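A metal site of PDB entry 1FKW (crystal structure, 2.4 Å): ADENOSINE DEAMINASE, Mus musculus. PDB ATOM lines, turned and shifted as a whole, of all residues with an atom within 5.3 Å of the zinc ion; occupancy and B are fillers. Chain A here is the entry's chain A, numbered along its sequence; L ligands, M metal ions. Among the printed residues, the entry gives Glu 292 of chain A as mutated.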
ATOM      1  N   HIS A  12     -27.435  -5.073 -15.001  1.00  0.00           N
ATOM      2  CA  HIS A  12     -26.922  -6.407 -14.710  1.00  0.00           C
ATOM      3  C   HIS A  12     -25.541  -6.545 -14.083  1.00  0.00           C
ATOM      4  O   HIS A  12     -24.561  -6.812 -14.788  1.00  0.00           O
ATOM      5  CB  HIS A  12     -26.922  -7.196 -16.006  1.00  0.00           C
ATOM      6  CG  HIS A  12     -27.038  -8.660 -15.808  1.00  0.00           C
ATOM      7  ND1 HIS A  12     -28.034  -9.377 -16.420  1.00  0.00           N
ATOM      8  CD2 HIS A  12     -26.402  -9.523 -14.984  1.00  0.00           C
ATOM      9  CE1 HIS A  12     -28.004 -10.625 -15.984  1.00  0.00           C
ATOM     10  NE2 HIS A  12     -27.036 -10.738 -15.101  1.00  0.00           N
ATOM     11  N   HIS A  14     -23.655  -8.258 -10.307  1.00  0.00           N
ATOM     12  CA  HIS A  14     -23.843  -8.905  -8.998  1.00  0.00           C
ATOM     13  C   HIS A  14     -22.992  -8.230  -7.944  1.00  0.00           C
ATOM     14  O   HIS A  14     -21.807  -8.020  -8.156  1.00  0.00           O
ATOM     15  CB  HIS A  14     -23.438 -10.362  -9.076  1.00  0.00           C
ATOM     16  CG  HIS A  14     -24.166 -11.150 -10.108  1.00  0.00           C
ATOM     17  ND1 HIS A  14     -25.121 -12.090  -9.786  1.00  0.00           N
ATOM     18  CD2 HIS A  14     -24.024 -11.211 -11.457  1.00  0.00           C
ATOM     19  CE1 HIS A  14     -25.527 -12.707 -10.893  1.00  0.00           C
ATOM     20  NE2 HIS A  14     -24.876 -12.185 -11.922  1.00  0.00           N
ATOM     21  N   ARG A  98     -27.598  -6.895  -8.122  1.00  0.00           N
ATOM     22  CA  ARG A  98     -28.258  -8.140  -7.718  1.00  0.00           C
ATOM     23  C   ARG A  98     -27.363  -9.022  -6.856  1.00  0.00           C
ATOM     24  O   ARG A  98     -26.145  -8.937  -6.907  1.00  0.00           O
ATOM     25  CB  ARG A  98     -28.735  -8.896  -8.937  1.00  0.00           C
ATOM     26  CG  ARG A  98     -27.666  -9.527  -9.797  1.00  0.00           C
ATOM     27  CD  ARG A  98     -28.311 -10.170 -10.993  1.00  0.00           C
ATOM     28  NE  ARG A  98     -28.903  -9.171 -11.863  1.00  0.00           N
ATOM     29  CZ  ARG A  98     -29.669  -9.447 -12.920  1.00  0.00           C
ATOM     30  NH1 ARG A  98     -30.034 -10.701 -13.170  1.00  0.00           N
ATOM     31  NH2 ARG A  98     -30.137  -8.467 -13.670  1.00  0.00           N
ATOM     32  N   HIS A 211     -31.821 -15.257 -15.619  1.00  0.00           N
ATOM     33  CA  HIS A 211     -30.609 -15.518 -16.402  1.00  0.00           C
ATOM     34  C   HIS A 211     -31.020 -16.656 -17.312  1.00  0.00           C
ATOM     35  O   HIS A 211     -31.557 -17.666 -16.820  1.00  0.00           O
ATOM     36  CB  HIS A 211     -29.457 -16.021 -15.523  1.00  0.00           C
ATOM     37  CG  HIS A 211     -28.749 -14.959 -14.748  1.00  0.00           C
ATOM     38  ND1 HIS A 211     -29.341 -14.277 -13.711  1.00  0.00           N
ATOM     39  CD2 HIS A 211     -27.465 -14.538 -14.801  1.00  0.00           C
ATOM     40  CE1 HIS A 211     -28.432 -13.486 -13.141  1.00  0.00           C
ATOM     41  NE2 HIS A 211     -27.285 -13.632 -13.785  1.00  0.00           N
ATOM     42  N   HIS A 235     -28.756 -12.110 -20.420  1.00  0.00           N
ATOM     43  CA  HIS A 235     -27.990 -12.734 -21.484  1.00  0.00           C
ATOM     44  C   HIS A 235     -28.855 -13.015 -22.712  1.00  0.00           C
ATOM     45  O   HIS A 235     -28.935 -12.189 -23.596  1.00  0.00           O
ATOM     46  CB  HIS A 235     -27.278 -14.010 -20.993  1.00  0.00           C
ATOM     47  CG  HIS A 235     -26.224 -13.763 -19.960  1.00  0.00           C
ATOM     48  ND1 HIS A 235     -25.097 -13.002 -20.224  1.00  0.00           N
ATOM     49  CD2 HIS A 235     -26.145 -14.114 -18.660  1.00  0.00           C
ATOM     50  CE1 HIS A 235     -24.370 -12.896 -19.113  1.00  0.00           C
ATOM     51  NE2 HIS A 235     -24.981 -13.567 -18.163  1.00  0.00           N
ATOM     52  N   GLU A 292     -21.756  -7.415 -15.393  1.00  0.00           N
ATOM     53  CA  GLU A 292     -22.063  -8.667 -14.693  1.00  0.00           C
ATOM     54  C   GLU A 292     -21.290  -9.008 -13.417  1.00  0.00           C
ATOM     55  O   GLU A 292     -21.909  -9.028 -12.343  1.00  0.00           O
ATOM     56  CB  GLU A 292     -22.249  -9.878 -15.605  1.00  0.00           C
ATOM     57  CG  GLU A 292     -23.203 -10.874 -14.914  1.00  0.00           C
ATOM     58  CD  GLU A 292     -23.355 -12.200 -15.599  1.00  0.00           C
ATOM     59  OE1 GLU A 292     -22.549 -12.468 -16.500  1.00  0.00           O
ATOM     60  OE2 GLU A 292     -24.296 -12.961 -15.232  1.00  0.00           O
ATOM     61  N   ASP A 293     -19.985  -9.273 -13.504  1.00  0.00           N
ATOM     62  CA  ASP A 293     -19.128  -9.595 -12.325  1.00  0.00           C
ATOM     63  C   ASP A 293     -17.758  -8.942 -12.623  1.00  0.00           C
ATOM     64  O   ASP A 293     -16.776  -9.626 -12.931  1.00  0.00           O
ATOM     65  CB  ASP A 293     -18.904 -11.113 -12.177  1.00  0.00           C
ATOM     66  CG  ASP A 293     -20.160 -11.884 -11.805  1.00  0.00           C
ATOM     67  OD1 ASP A 293     -20.561 -11.849 -10.635  1.00  0.00           O
ATOM     68  OD2 ASP A 293     -20.725 -12.585 -12.683  1.00  0.00           O
HETATM   69  N1  LIG L   1     -24.182 -16.439 -14.452  1.00  0.00           N
HETATM   70  C1  LIG L   1     -24.957 -17.103 -13.605  1.00  0.00           C
HETATM   71  N2  LIG L   1     -24.917 -16.898 -12.282  1.00  0.00           N
HETATM   72  C2  LIG L   1     -24.046 -15.994 -11.762  1.00  0.00           C
HETATM   73  C3  LIG L   1     -23.224 -15.297 -12.581  1.00  0.00           C
HETATM   74  C4  LIG L   1     -23.268 -15.502 -13.995  1.00  0.00           C
HETATM   75  N3  LIG L   1     -22.485 -14.479 -11.806  1.00  0.00           N
HETATM   76  C5  LIG L   1     -22.832 -14.679 -10.536  1.00  0.00           C
HETATM   77  N4  LIG L   1     -23.791 -15.599 -10.490  1.00  0.00           N
HETATM   78  C6  LIG L   1     -24.358 -16.153  -9.302  1.00  0.00           C
HETATM   79  C7  LIG L   1     -23.227 -16.282  -8.281  1.00  0.00           C
HETATM   80  O1  LIG L   1     -23.170 -17.631  -7.804  1.00  0.00           O
HETATM   81  C8  LIG L   1     -23.429 -15.255  -7.122  1.00  0.00           C
HETATM   82  O2  LIG L   1     -23.151 -15.855  -5.842  1.00  0.00           O
HETATM   83  C9  LIG L   1     -25.006 -15.146  -7.401  1.00  0.00           C
HETATM   84  O3  LIG L   1     -25.275 -15.238  -8.753  1.00  0.00           O
HETATM   85  C10 LIG L   1     -25.628 -13.843  -6.829  1.00  0.00           C
HETATM   86  O4  LIG L   1     -24.949 -12.642  -7.284  1.00  0.00           O
HETATM   87 ZN    ZN M   1     -25.627 -12.388 -13.996  1.00  0.00          ZN
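A ring nitrogen (ND1) of His 14 lies within hydrogen-bond range of an oxygen (O4) of the ligand, at 2.6 Å. The side-chain carboxylate (OD2) of Asp 293 sits at hydrogen-bond distance from a nitrogen (N3) of the ligand, at 2.7 Å.
The side-chain carboxylate of Glu 292 is in hydrogen-bond range of a ring nitrogen (NE2) of His 235, 3.1 Å away.
The zinc ion is bound by OE2 of Glu 292, NE2 of His 211, NE2 of His 14 and NE2 of His 12. The zinc ion has four donor atoms within binding distance.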
